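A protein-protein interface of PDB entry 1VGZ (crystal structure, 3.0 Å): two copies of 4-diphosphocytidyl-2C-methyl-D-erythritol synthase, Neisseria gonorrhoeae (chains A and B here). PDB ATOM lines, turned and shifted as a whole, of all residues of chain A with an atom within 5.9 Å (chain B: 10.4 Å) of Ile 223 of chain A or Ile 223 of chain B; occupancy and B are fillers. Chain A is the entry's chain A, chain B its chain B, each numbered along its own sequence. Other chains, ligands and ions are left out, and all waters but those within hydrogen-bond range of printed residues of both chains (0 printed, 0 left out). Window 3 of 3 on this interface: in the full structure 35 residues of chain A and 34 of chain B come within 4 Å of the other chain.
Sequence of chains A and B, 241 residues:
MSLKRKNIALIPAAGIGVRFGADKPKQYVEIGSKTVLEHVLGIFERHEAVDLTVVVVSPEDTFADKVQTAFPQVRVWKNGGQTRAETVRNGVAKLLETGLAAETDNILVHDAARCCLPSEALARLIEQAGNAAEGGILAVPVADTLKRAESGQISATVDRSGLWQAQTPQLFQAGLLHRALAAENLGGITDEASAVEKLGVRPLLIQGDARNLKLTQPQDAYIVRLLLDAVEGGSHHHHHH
OD1 of Asp 209 of chain B lies within salt-bridge range of NH2 of Arg 211 of chain B (2.8 Å).
Among the printed residues, pairs that only touch across the chains: Ala 210 of chain A with Ile 223 of chain B, Arg 211 of chain A with Ile 223 of chain B, Ile 223 of chain A with Ala 210 of chain B, Ile 223 of chain A with Arg 211 of chain B, Ile 223 of chain A with Ile 223 of chain B and Leu 226 of chain A with Leu 226 of chain B.
Of chain B, only Ala 210 (3.5 Å), Arg 211 (3.8 Å) and Ile 223 (3.9 Å) come within 4 Å of Ile 223 of chain A. Ile 223 of chain B touches just these residues of chain A: Ala 210 (3.7 Å), Arg 211 (3.9 Å) and Ile 223 (3.9 Å). Ala 210 of chain A touches just one residue of chain B: Ile 223 (3.7 Å). Ala 221 of chain A touches none of the printed residues of chain B. No residue of chain B comes within 4 Å of Val 224 of chain A. Leu 226 of chain A touches one residue of chain B. No residue of chain B comes within 4 Å of Leu 227 of chain A. Of the printed residues of chain A, Leu 226 of chain B touches Leu 226. Printed residues of chain A within 4 Å of Ala 210 of chain B: Ile 223. Printed residues of chain A within 4 Å of Arg 211 of chain B: Ile 223 (3.8 Å). Of the printed residues of chain B, Arg 211 of chain A touches Ile 223 (3.9 Å). The nearest residue of chain B that does not touch Ile 223 of chain A is Leu 227 of chain B (4.8 Å).
Of the 14 printed residues of chain A, 4 touch a printed residue of chain B. Hydrophobic or aromatic side chains of chain A within 4 Å of the printed part of chain B: Ala 210, Ile 223 and Leu 226. Printed residues of chain B that touch a printed residue of chain A: Ala 210, Arg 211, Ile 223 and Leu 226.
Ala 210 of chain A touches Ile 223 of chain B, and with the chains exchanged Ile 223 of chain A touches Ala 210 of chain B. Arg 211 of chain A touches Ile 223 of chain B, and with the chains exchanged Ile 223 of chain A touches Arg 211 of chain B. Ile 223 of chain A touches its own counterpart, Ile 223 of chain B. Leu 226 of chain B touches its own counterpart, Leu 226 of chain A.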
ATOM      1  N   CYS A 116       6.101 -14.674  -2.539  1.00  0.00           N
ATOM      2  CA  CYS A 116       5.195 -15.031  -3.632  1.00  0.00           C
ATOM      3  C   CYS A 116       4.917 -16.530  -3.596  1.00  0.00           C
ATOM      4  O   CYS A 116       4.980 -17.253  -4.591  1.00  0.00           O
ATOM      5  CB  CYS A 116       5.772 -14.604  -4.977  1.00  0.00           C
ATOM      6  SG  CYS A 116       6.006 -12.823  -5.136  1.00  0.00           S
ATOM      7  N   ALA A 210       7.495 -21.905  -9.546  1.00  0.00           N
ATOM      8  CA  ALA A 210       8.397 -20.989 -10.241  1.00  0.00           C
ATOM      9  C   ALA A 210       8.270 -19.583  -9.669  1.00  0.00           C
ATOM     10  O   ALA A 210       9.245 -18.857  -9.507  1.00  0.00           O
ATOM     11  CB  ALA A 210       8.122 -20.972 -11.735  1.00  0.00           C
ATOM     12  N   ARG A 211       7.041 -19.226  -9.310  1.00  0.00           N
ATOM     13  CA  ARG A 211       6.718 -17.946  -8.725  1.00  0.00           C
ATOM     14  C   ARG A 211       7.213 -17.823  -7.290  1.00  0.00           C
ATOM     15  O   ARG A 211       7.227 -16.713  -6.761  1.00  0.00           O
ATOM     16  CB  ARG A 211       5.213 -17.728  -8.688  1.00  0.00           C
ATOM     17  CG  ARG A 211       4.533 -17.706 -10.037  1.00  0.00           C
ATOM     18  CD  ARG A 211       3.028 -17.752  -9.792  1.00  0.00           C
ATOM     19  NE  ARG A 211       2.502 -19.103  -9.996  1.00  0.00           N
ATOM     20  CZ  ARG A 211       1.369 -19.480  -9.403  1.00  0.00           C
ATOM     21  NH1 ARG A 211       0.743 -18.606  -8.621  1.00  0.00           N
ATOM     22  NH2 ARG A 211       0.850 -20.684  -9.565  1.00  0.00           N
ATOM     23  N   LEU A 213       9.906 -17.469  -5.736  1.00  0.00           N
ATOM     24  CA  LEU A 213      11.276 -17.030  -5.892  1.00  0.00           C
ATOM     25  C   LEU A 213      11.691 -16.131  -4.734  1.00  0.00           C
ATOM     26  O   LEU A 213      10.889 -15.383  -4.180  1.00  0.00           O
ATOM     27  CB  LEU A 213      11.472 -16.311  -7.226  1.00  0.00           C
ATOM     28  CG  LEU A 213      10.858 -14.912  -7.350  1.00  0.00           C
ATOM     29  CD1 LEU A 213      11.877 -13.853  -6.948  1.00  0.00           C
ATOM     30  CD2 LEU A 213      10.335 -14.674  -8.757  1.00  0.00           C
ATOM     31  N   GLN A 219      16.916  -7.268  -9.822  1.00  0.00           N
ATOM     32  CA  GLN A 219      16.263  -7.871 -10.968  1.00  0.00           C
ATOM     33  C   GLN A 219      15.096  -8.750 -10.540  1.00  0.00           C
ATOM     34  O   GLN A 219      14.188  -9.002 -11.337  1.00  0.00           O
ATOM     35  CB  GLN A 219      17.287  -8.657 -11.797  1.00  0.00           C
ATOM     36  N   ASP A 220      15.092  -9.246  -9.307  1.00  0.00           N
ATOM     37  CA  ASP A 220      14.024 -10.087  -8.788  1.00  0.00           C
ATOM     38  C   ASP A 220      12.806  -9.260  -8.370  1.00  0.00           C
ATOM     39  O   ASP A 220      11.657  -9.680  -8.543  1.00  0.00           O
ATOM     40  CB  ASP A 220      14.477 -10.887  -7.576  1.00  0.00           C
ATOM     41  CG  ASP A 220      15.555 -11.908  -7.816  1.00  0.00           C
ATOM     42  OD1 ASP A 220      15.300 -12.914  -8.513  1.00  0.00           O
ATOM     43  OD2 ASP A 220      16.670 -11.715  -7.273  1.00  0.00           O
ATOM     44  N   ALA A 221      13.066  -8.084  -7.798  1.00  0.00           N
ATOM     45  CA  ALA A 221      11.972  -7.201  -7.377  1.00  0.00           C
ATOM     46  C   ALA A 221      11.020  -6.950  -8.546  1.00  0.00           C
ATOM     47  O   ALA A 221       9.803  -7.031  -8.376  1.00  0.00           O
ATOM     48  CB  ALA A 221      12.518  -5.898  -6.824  1.00  0.00           C
ATOM     49  N   TYR A 222      11.571  -6.685  -9.735  1.00  0.00           N
ATOM     50  CA  TYR A 222      10.776  -6.468 -10.945  1.00  0.00           C
ATOM     51  C   TYR A 222       9.742  -7.587 -11.071  1.00  0.00           C
ATOM     52  O   TYR A 222       8.541  -7.340 -11.067  1.00  0.00           O
ATOM     53  CB  TYR A 222      11.676  -6.460 -12.171  1.00  0.00           C
ATOM     54  CG  TYR A 222      11.128  -5.935 -13.471  1.00  0.00           C
ATOM     55  CD1 TYR A 222      11.380  -4.617 -13.853  1.00  0.00           C
ATOM     56  CD2 TYR A 222      10.396  -6.727 -14.344  1.00  0.00           C
ATOM     57  CE1 TYR A 222      10.904  -4.101 -15.045  1.00  0.00           C
ATOM     58  CE2 TYR A 222       9.914  -6.226 -15.539  1.00  0.00           C
ATOM     59  CZ  TYR A 222      10.174  -4.916 -15.886  1.00  0.00           C
ATOM     60  OH  TYR A 222       9.697  -4.425 -17.082  1.00  0.00           O
ATOM     61  N   ILE A 223      10.233  -8.830 -11.124  1.00  0.00           N
ATOM     62  CA  ILE A 223       9.340  -9.969 -11.222  1.00  0.00           C
ATOM     63  C   ILE A 223       8.399 -10.065 -10.024  1.00  0.00           C
ATOM     64  O   ILE A 223       7.216 -10.365 -10.231  1.00  0.00           O
ATOM     65  CB  ILE A 223      10.068 -11.319 -11.376  1.00  0.00           C
ATOM     66  CG1 ILE A 223      11.163 -11.233 -12.440  1.00  0.00           C
ATOM     67  CG2 ILE A 223       9.057 -12.407 -11.746  1.00  0.00           C
ATOM     68  CD1 ILE A 223      11.999 -12.487 -12.588  1.00  0.00           C
ATOM     69  N   VAL A 224       8.886  -9.826  -8.809  1.00  0.00           N
ATOM     70  CA  VAL A 224       8.020  -9.939  -7.628  1.00  0.00           C
ATOM     71  C   VAL A 224       6.873  -8.942  -7.642  1.00  0.00           C
ATOM     72  O   VAL A 224       5.702  -9.340  -7.608  1.00  0.00           O
ATOM     73  CB  VAL A 224       8.802  -9.823  -6.312  1.00  0.00           C
ATOM     74  N   ARG A 225       7.190  -7.658  -7.785  1.00  0.00           N
ATOM     75  CA  ARG A 225       6.191  -6.592  -7.846  1.00  0.00           C
ATOM     76  C   ARG A 225       5.115  -6.962  -8.863  1.00  0.00           C
ATOM     77  O   ARG A 225       3.922  -7.089  -8.586  1.00  0.00           O
ATOM     78  CB  ARG A 225       6.872  -5.273  -8.223  1.00  0.00           C
ATOM     79  CG  ARG A 225       7.932  -4.829  -7.220  1.00  0.00           C
ATOM     80  CD  ARG A 225       8.806  -3.718  -7.759  1.00  0.00           C
ATOM     81  NE  ARG A 225       9.298  -2.824  -6.723  1.00  0.00           N
ATOM     82  CZ  ARG A 225       8.550  -1.915  -6.100  1.00  0.00           C
ATOM     83  NH1 ARG A 225       9.091  -1.138  -5.162  1.00  0.00           N
ATOM     84  NH2 ARG A 225       7.263  -1.785  -6.393  1.00  0.00           N
ATOM     85  N   LEU A 226       5.593  -7.384 -10.031  1.00  0.00           N
ATOM     86  CA  LEU A 226       4.796  -7.840 -11.148  1.00  0.00           C
ATOM     87  C   LEU A 226       3.951  -9.055 -10.788  1.00  0.00           C
ATOM     88  O   LEU A 226       2.953  -9.346 -11.452  1.00  0.00           O
ATOM     89  CB  LEU A 226       5.734  -8.156 -12.317  1.00  0.00           C
ATOM     90  CG  LEU A 226       5.142  -8.336 -13.705  1.00  0.00           C
ATOM     91  CD1 LEU A 226       3.989  -7.371 -13.957  1.00  0.00           C
ATOM     92  CD2 LEU A 226       6.221  -8.158 -14.773  1.00  0.00           C
ATOM     93  N   LEU A 227       4.374  -9.826  -9.789  1.00  0.00           N
ATOM     94  CA  LEU A 227       3.651 -11.000  -9.333  1.00  0.00           C
ATOM     95  C   LEU A 227       2.569 -10.610  -8.338  1.00  0.00           C
ATOM     96  O   LEU A 227       1.488 -11.210  -8.314  1.00  0.00           O
ATOM     97  CB  LEU A 227       4.596 -12.038  -8.728  1.00  0.00           C
ATOM     98  CG  LEU A 227       5.231 -12.991  -9.751  1.00  0.00           C
ATOM     99  CD1 LEU A 227       6.411 -13.718  -9.142  1.00  0.00           C
ATOM    100  CD2 LEU A 227       4.196 -13.948 -10.315  1.00  0.00           C
ATOM    101  N   LEU A 228       2.846  -9.569  -7.549  1.00  0.00           N
ATOM    102  CA  LEU A 228       1.864  -9.093  -6.569  1.00  0.00           C
ATOM    103  C   LEU A 228       0.948  -8.044  -7.195  1.00  0.00           C
ATOM    104  O   LEU A 228       0.901  -6.881  -6.784  1.00  0.00           O
ATOM    105  CB  LEU A 228       2.571  -8.561  -5.326  1.00  0.00           C
ATOM    106  N   ILE B  31       0.411 -16.300 -26.957  1.00  0.00           N
ATOM    107  CA  ILE B  31       0.561 -15.428 -25.787  1.00  0.00           C
ATOM    108  C   ILE B  31       0.623 -13.991 -26.296  1.00  0.00           C
ATOM    109  O   ILE B  31       1.272 -13.755 -27.325  1.00  0.00           O
ATOM    110  CB  ILE B  31       1.794 -15.764 -24.948  1.00  0.00           C
ATOM    111  N   ALA B 113      11.945 -21.361 -26.780  1.00  0.00           N
ATOM    112  CA  ALA B 113      11.056 -20.980 -25.715  1.00  0.00           C
ATOM    113  C   ALA B 113      11.496 -19.906 -24.746  1.00  0.00           C
ATOM    114  O   ALA B 113      10.697 -19.636 -23.811  1.00  0.00           O
ATOM    115  CB  ALA B 113      10.686 -22.232 -24.887  1.00  0.00           C
ATOM    116  N   CYS B 115      11.387 -16.609 -24.508  1.00  0.00           N
ATOM    117  CA  CYS B 115      10.857 -15.420 -25.142  1.00  0.00           C
ATOM    118  C   CYS B 115      10.743 -14.226 -24.223  1.00  0.00           C
ATOM    119  O   CYS B 115       9.710 -13.542 -24.265  1.00  0.00           O
ATOM    120  CB  CYS B 115       9.467 -15.751 -25.726  1.00  0.00           C
ATOM    121  SG  CYS B 115       8.538 -16.900 -24.673  1.00  0.00           S
ATOM    122  N   CYS B 116      11.684 -14.002 -23.317  1.00  0.00           N
ATOM    123  CA  CYS B 116      11.633 -12.852 -22.417  1.00  0.00           C
ATOM    124  C   CYS B 116      13.063 -12.361 -22.166  1.00  0.00           C
ATOM    125  O   CYS B 116      13.403 -11.860 -21.098  1.00  0.00           O
ATOM    126  CB  CYS B 116      10.954 -13.186 -21.103  1.00  0.00           C
ATOM    127  SG  CYS B 116       9.307 -13.897 -21.168  1.00  0.00           S
ATOM    128  N   PRO B 118      15.875 -10.036 -21.996  1.00  0.00           N
ATOM    129  CA  PRO B 118      16.071  -8.600 -21.922  1.00  0.00           C
ATOM    130  C   PRO B 118      16.995  -8.111 -23.027  1.00  0.00           C
ATOM    131  O   PRO B 118      17.847  -8.857 -23.514  1.00  0.00           O
ATOM    132  CB  PRO B 118      16.662  -8.384 -20.537  1.00  0.00           C
ATOM    133  CG  PRO B 118      16.257  -9.559 -19.739  1.00  0.00           C
ATOM    134  CD  PRO B 118      16.168 -10.708 -20.711  1.00  0.00           C
ATOM    135  N   VAL B 140      23.089 -17.308 -14.608  1.00  0.00           N
ATOM    136  CA  VAL B 140      22.831 -16.711 -13.291  1.00  0.00           C
ATOM    137  C   VAL B 140      23.344 -17.686 -12.234  1.00  0.00           C
ATOM    138  O   VAL B 140      23.317 -18.887 -12.477  1.00  0.00           O
ATOM    139  CB  VAL B 140      21.358 -16.401 -13.043  1.00  0.00           C
ATOM    140  CG1 VAL B 140      20.814 -15.399 -14.064  1.00  0.00           C
ATOM    141  CG2 VAL B 140      20.514 -17.677 -13.100  1.00  0.00           C
ATOM    142  N   GLN B 167      22.014 -20.236 -19.356  1.00  0.00           N
ATOM    143  CA  GLN B 167      20.866 -19.758 -20.120  1.00  0.00           C
ATOM    144  C   GLN B 167      21.282 -19.618 -21.585  1.00  0.00           C
ATOM    145  O   GLN B 167      22.336 -20.160 -21.940  1.00  0.00           O
ATOM    146  CB  GLN B 167      20.445 -18.357 -19.635  1.00  0.00           C
ATOM    147  CG  GLN B 167      20.077 -18.352 -18.165  1.00  0.00           C
ATOM    148  CD  GLN B 167      19.552 -17.022 -17.692  1.00  0.00           C
ATOM    149  OE1 GLN B 167      20.062 -15.973 -18.103  1.00  0.00           O
ATOM    150  NE2 GLN B 167      18.536 -17.079 -16.830  1.00  0.00           N
ATOM    151  N   GLY B 208      23.255 -13.529 -16.747  1.00  0.00           N
ATOM    152  CA  GLY B 208      22.065 -13.706 -17.590  1.00  0.00           C
ATOM    153  C   GLY B 208      20.950 -12.812 -17.042  1.00  0.00           C
ATOM    154  O   GLY B 208      21.181 -11.622 -16.818  1.00  0.00           O
ATOM    155  N   ASP B 209      19.768 -13.392 -16.831  1.00  0.00           N
ATOM    156  CA  ASP B 209      18.660 -12.616 -16.278  1.00  0.00           C
ATOM    157  C   ASP B 209      17.581 -13.516 -15.684  1.00  0.00           C
ATOM    158  O   ASP B 209      17.310 -14.599 -16.207  1.00  0.00           O
ATOM    159  CB  ASP B 209      18.045 -11.683 -17.302  1.00  0.00           C
ATOM    160  CG  ASP B 209      17.351 -10.478 -16.681  1.00  0.00           C
ATOM    161  OD1 ASP B 209      17.819  -9.345 -16.987  1.00  0.00           O
ATOM    162  OD2 ASP B 209      16.366 -10.662 -15.937  1.00  0.00           O
ATOM    163  N   ALA B 210      16.958 -13.041 -14.608  1.00  0.00           N
ATOM    164  CA  ALA B 210      15.903 -13.786 -13.933  1.00  0.00           C
ATOM    165  C   ALA B 210      14.690 -13.972 -14.835  1.00  0.00           C
ATOM    166  O   ALA B 210      14.107 -15.053 -14.885  1.00  0.00           O
ATOM    167  CB  ALA B 210      15.485 -13.060 -12.661  1.00  0.00           C
ATOM    168  N   ARG B 211      14.363 -12.934 -15.606  1.00  0.00           N
ATOM    169  CA  ARG B 211      13.252 -12.950 -16.523  1.00  0.00           C
ATOM    170  C   ARG B 211      13.535 -13.760 -17.785  1.00  0.00           C
ATOM    171  O   ARG B 211      12.614 -13.911 -18.587  1.00  0.00           O
ATOM    172  CB  ARG B 211      12.831 -11.569 -17.007  1.00  0.00           C
ATOM    173  CG  ARG B 211      12.456 -10.576 -15.945  1.00  0.00           C
ATOM    174  CD  ARG B 211      13.539  -9.523 -15.797  1.00  0.00           C
ATOM    175  NE  ARG B 211      13.418  -8.473 -16.817  1.00  0.00           N
ATOM    176  CZ  ARG B 211      14.416  -7.609 -17.021  1.00  0.00           C
ATOM    177  NH1 ARG B 211      14.303  -6.653 -17.924  1.00  0.00           N
ATOM    178  NH2 ARG B 211      15.558  -7.742 -16.351  1.00  0.00           N
ATOM    179  N   ASN B 212      14.776 -14.146 -18.001  1.00  0.00           N
ATOM    180  CA  ASN B 212      15.163 -14.935 -19.182  1.00  0.00           C
ATOM    181  C   ASN B 212      15.059 -16.414 -18.814  1.00  0.00           C
ATOM    182  O   ASN B 212      16.035 -17.124 -18.619  1.00  0.00           O
ATOM    183  CB  ASN B 212      16.547 -14.513 -19.624  1.00  0.00           C
ATOM    184  CG  ASN B 212      17.182 -15.276 -20.749  1.00  0.00           C
ATOM    185  OD1 ASN B 212      16.645 -15.473 -21.836  1.00  0.00           O
ATOM    186  ND2 ASN B 212      18.402 -15.735 -20.473  1.00  0.00           N
ATOM    187  N   LEU B 213      13.814 -16.836 -18.622  1.00  0.00           N
ATOM    188  CA  LEU B 213      13.448 -18.171 -18.215  1.00  0.00           C
ATOM    189  C   LEU B 213      12.899 -18.963 -19.391  1.00  0.00           C
ATOM    190  O   LEU B 213      12.302 -18.410 -20.310  1.00  0.00           O
ATOM    191  CB  LEU B 213      12.387 -18.116 -17.103  1.00  0.00           C
ATOM    192  CG  LEU B 213      11.001 -17.614 -17.527  1.00  0.00           C
ATOM    193  CD1 LEU B 213      10.094 -18.765 -17.934  1.00  0.00           C
ATOM    194  CD2 LEU B 213      10.373 -16.783 -16.425  1.00  0.00           C
ATOM    195  N   LYS B 214      13.042 -20.269 -19.323  1.00  0.00           N
ATOM    196  CA  LYS B 214      12.553 -21.132 -20.408  1.00  0.00           C
ATOM    197  C   LYS B 214      11.138 -21.585 -20.113  1.00  0.00           C
ATOM    198  O   LYS B 214      10.825 -21.953 -18.975  1.00  0.00           O
ATOM    199  CB  LYS B 214      13.521 -22.298 -20.508  1.00  0.00           C
ATOM    200  CG  LYS B 214      13.483 -23.160 -21.744  1.00  0.00           C
ATOM    201  CD  LYS B 214      14.650 -24.150 -21.707  1.00  0.00           C
ATOM    202  CE  LYS B 214      14.790 -24.864 -23.040  1.00  0.00           C
ATOM    203  NZ  LYS B 214      13.556 -25.635 -23.380  1.00  0.00           N
ATOM    204  N   LEU B 215      10.236 -21.470 -21.074  1.00  0.00           N
ATOM    205  CA  LEU B 215       8.848 -21.881 -20.892  1.00  0.00           C
ATOM    206  C   LEU B 215       8.721 -23.390 -21.075  1.00  0.00           C
ATOM    207  O   LEU B 215       8.489 -23.905 -22.164  1.00  0.00           O
ATOM    208  CB  LEU B 215       7.924 -21.154 -21.863  1.00  0.00           C
ATOM    209  CG  LEU B 215       6.527 -21.748 -22.064  1.00  0.00           C
ATOM    210  CD1 LEU B 215       5.696 -21.559 -20.813  1.00  0.00           C
ATOM    211  CD2 LEU B 215       5.849 -21.134 -23.280  1.00  0.00           C
ATOM    212  N   THR B 216       8.892 -24.111 -19.977  1.00  0.00           N
ATOM    213  CA  THR B 216       8.789 -25.564 -19.987  1.00  0.00           C
ATOM    214  C   THR B 216       7.435 -26.005 -19.433  1.00  0.00           C
ATOM    215  O   THR B 216       6.649 -26.683 -20.109  1.00  0.00           O
ATOM    216  CB  THR B 216       9.927 -26.199 -19.169  1.00  0.00           C
ATOM    217  N   GLN B 217       7.114 -25.578 -18.211  1.00  0.00           N
ATOM    218  CA  GLN B 217       5.845 -25.958 -17.605  1.00  0.00           C
ATOM    219  C   GLN B 217       4.759 -24.904 -17.750  1.00  0.00           C
ATOM    220  O   GLN B 217       5.014 -23.701 -17.831  1.00  0.00           O
ATOM    221  CB  GLN B 217       6.044 -26.238 -16.108  1.00  0.00           C
ATOM    222  CG  GLN B 217       6.390 -27.671 -15.768  1.00  0.00           C
ATOM    223  CD  GLN B 217       7.814 -28.053 -16.114  1.00  0.00           C
ATOM    224  OE1 GLN B 217       8.028 -28.888 -16.999  1.00  0.00           O
ATOM    225  NE2 GLN B 217       8.780 -27.461 -15.424  1.00  0.00           N
ATOM    226  N   PRO B 218       3.516 -25.344 -17.536  1.00  0.00           N
ATOM    227  CA  PRO B 218       2.344 -24.472 -17.591  1.00  0.00           C
ATOM    228  C   PRO B 218       2.500 -23.337 -16.593  1.00  0.00           C
ATOM    229  O   PRO B 218       2.174 -22.178 -16.852  1.00  0.00           O
ATOM    230  CB  PRO B 218       1.185 -25.392 -17.252  1.00  0.00           C
ATOM    231  CG  PRO B 218       1.647 -26.745 -17.705  1.00  0.00           C
ATOM    232  CD  PRO B 218       3.124 -26.770 -17.375  1.00  0.00           C
ATOM    233  N   GLN B 219       3.110 -23.666 -15.453  1.00  0.00           N
ATOM    234  CA  GLN B 219       3.403 -22.714 -14.398  1.00  0.00           C
ATOM    235  C   GLN B 219       4.308 -21.592 -14.896  1.00  0.00           C
ATOM    236  O   GLN B 219       4.253 -20.473 -14.378  1.00  0.00           O
ATOM    237  CB  GLN B 219       4.024 -23.440 -13.198  1.00  0.00           C
ATOM    238  N   ASP B 220       5.147 -21.846 -15.897  1.00  0.00           N
ATOM    239  CA  ASP B 220       6.050 -20.871 -16.479  1.00  0.00           C
ATOM    240  C   ASP B 220       5.326 -19.908 -17.432  1.00  0.00           C
ATOM    241  O   ASP B 220       5.763 -18.778 -17.676  1.00  0.00           O
ATOM    242  CB  ASP B 220       7.144 -21.545 -17.304  1.00  0.00           C
ATOM    243  CG  ASP B 220       8.141 -22.336 -16.500  1.00  0.00           C
ATOM    244  OD1 ASP B 220       8.851 -21.731 -15.670  1.00  0.00           O
ATOM    245  OD2 ASP B 220       8.208 -23.565 -16.735  1.00  0.00           O
ATOM    246  N   ALA B 221       4.291 -20.435 -18.090  1.00  0.00           N
ATOM    247  CA  ALA B 221       3.509 -19.599 -19.006  1.00  0.00           C
ATOM    248  C   ALA B 221       2.993 -18.380 -18.237  1.00  0.00           C
ATOM    249  O   ALA B 221       3.167 -17.250 -18.692  1.00  0.00           O
ATOM    250  CB  ALA B 221       2.371 -20.388 -19.616  1.00  0.00           C
ATOM    251  N   TYR B 222       2.390 -18.619 -17.065  1.00  0.00           N
ATOM    252  CA  TYR B 222       1.875 -17.530 -16.247  1.00  0.00           C
ATOM    253  C   TYR B 222       2.907 -16.425 -16.086  1.00  0.00           C
ATOM    254  O   TYR B 222       2.676 -15.297 -16.543  1.00  0.00           O
ATOM    255  CB  TYR B 222       1.412 -18.056 -14.893  1.00  0.00           C
ATOM    256  N   ILE B 223       4.088 -16.723 -15.527  1.00  0.00           N
ATOM    257  CA  ILE B 223       5.091 -15.682 -15.380  1.00  0.00           C
ATOM    258  C   ILE B 223       5.469 -15.073 -16.736  1.00  0.00           C
ATOM    259  O   ILE B 223       5.681 -13.853 -16.772  1.00  0.00           O
ATOM    260  CB  ILE B 223       6.404 -16.071 -14.694  1.00  0.00           C
ATOM    261  CG1 ILE B 223       6.246 -17.035 -13.521  1.00  0.00           C
ATOM    262  CG2 ILE B 223       7.104 -14.795 -14.192  1.00  0.00           C
ATOM    263  CD1 ILE B 223       7.590 -17.475 -12.944  1.00  0.00           C
ATOM    264  N   VAL B 224       5.583 -15.850 -17.811  1.00  0.00           N
ATOM    265  CA  VAL B 224       5.957 -15.267 -19.103  1.00  0.00           C
ATOM    266  C   VAL B 224       4.925 -14.281 -19.624  1.00  0.00           C
ATOM    267  O   VAL B 224       5.254 -13.122 -19.913  1.00  0.00           O
ATOM    268  CB  VAL B 224       6.237 -16.313 -20.192  1.00  0.00           C
ATOM    269  N   ARG B 225       3.660 -14.707 -19.675  1.00  0.00           N
ATOM    270  CA  ARG B 225       2.566 -13.855 -20.139  1.00  0.00           C
ATOM    271  C   ARG B 225       2.571 -12.546 -19.355  1.00  0.00           C
ATOM    272  O   ARG B 225       2.462 -11.458 -19.909  1.00  0.00           O
ATOM    273  CB  ARG B 225       1.222 -14.565 -20.007  1.00  0.00           C
ATOM    274  N   LEU B 226       2.766 -12.661 -18.044  1.00  0.00           N
ATOM    275  CA  LEU B 226       2.836 -11.542 -17.134  1.00  0.00           C
ATOM    276  C   LEU B 226       4.041 -10.655 -17.436  1.00  0.00           C
ATOM    277  O   LEU B 226       4.023  -9.452 -17.168  1.00  0.00           O
ATOM    278  CB  LEU B 226       2.920 -12.030 -15.680  1.00  0.00           C
ATOM    279  N   LEU B 227       5.105 -11.253 -17.966  1.00  0.00           N
ATOM    280  CA  LEU B 227       6.327 -10.548 -18.312  1.00  0.00           C
ATOM    281  C   LEU B 227       6.163  -9.785 -19.628  1.00  0.00           C
ATOM    282  O   LEU B 227       6.524  -8.612 -19.721  1.00  0.00           O
ATOM    283  CB  LEU B 227       7.504 -11.512 -18.463  1.00  0.00           C
ATOM    284  CG  LEU B 227       8.323 -11.794 -17.206  1.00  0.00           C
ATOM    285  CD1 LEU B 227       9.295 -12.934 -17.465  1.00  0.00           C
ATOM    286  CD2 LEU B 227       9.029 -10.549 -16.699  1.00  0.00           C
ATOM    287  N   LEU B 228       5.643 -10.509 -20.621  1.00  0.00           N
ATOM    288  CA  LEU B 228       5.437  -9.887 -21.933  1.00  0.00           C
ATOM    289  C   LEU B 228       4.480  -8.708 -21.807  1.00  0.00           C
ATOM    290  O   LEU B 228       4.884  -7.543 -21.884  1.00  0.00           O
ATOM    291  CB  LEU B 228       4.901 -10.936 -22.906  1.00  0.00           C
ATOM    292  CG  LEU B 228       5.736 -12.217 -23.020  1.00  0.00           C
ATOM    293  CD1 LEU B 228       4.843 -13.398 -23.362  1.00  0.00           C
ATOM    294  CD2 LEU B 228       6.830 -12.058 -24.065  1.00  0.00           C
ATOM    295  N   ASP B 229       3.219  -9.017 -21.528  1.00  0.00           N
ATOM    296  CA  ASP B 229       2.185  -7.998 -21.381  1.00  0.00           C
ATOM    297  C   ASP B 229       2.386  -7.170 -20.121  1.00  0.00           C
ATOM    298  O   ASP B 229       3.243  -6.285 -20.084  1.00  0.00           O
ATOM    299  CB  ASP B 229       0.795  -8.655 -21.375  1.00  0.00           C
ATOM    300  CG  ASP B 229       0.638  -9.637 -22.529  1.00  0.00           C
ATOM    301  OD1 ASP B 229       0.908  -9.226 -23.683  1.00  0.00           O
ATOM    302  OD2 ASP B 229       0.253 -10.802 -22.273  1.00  0.00           O
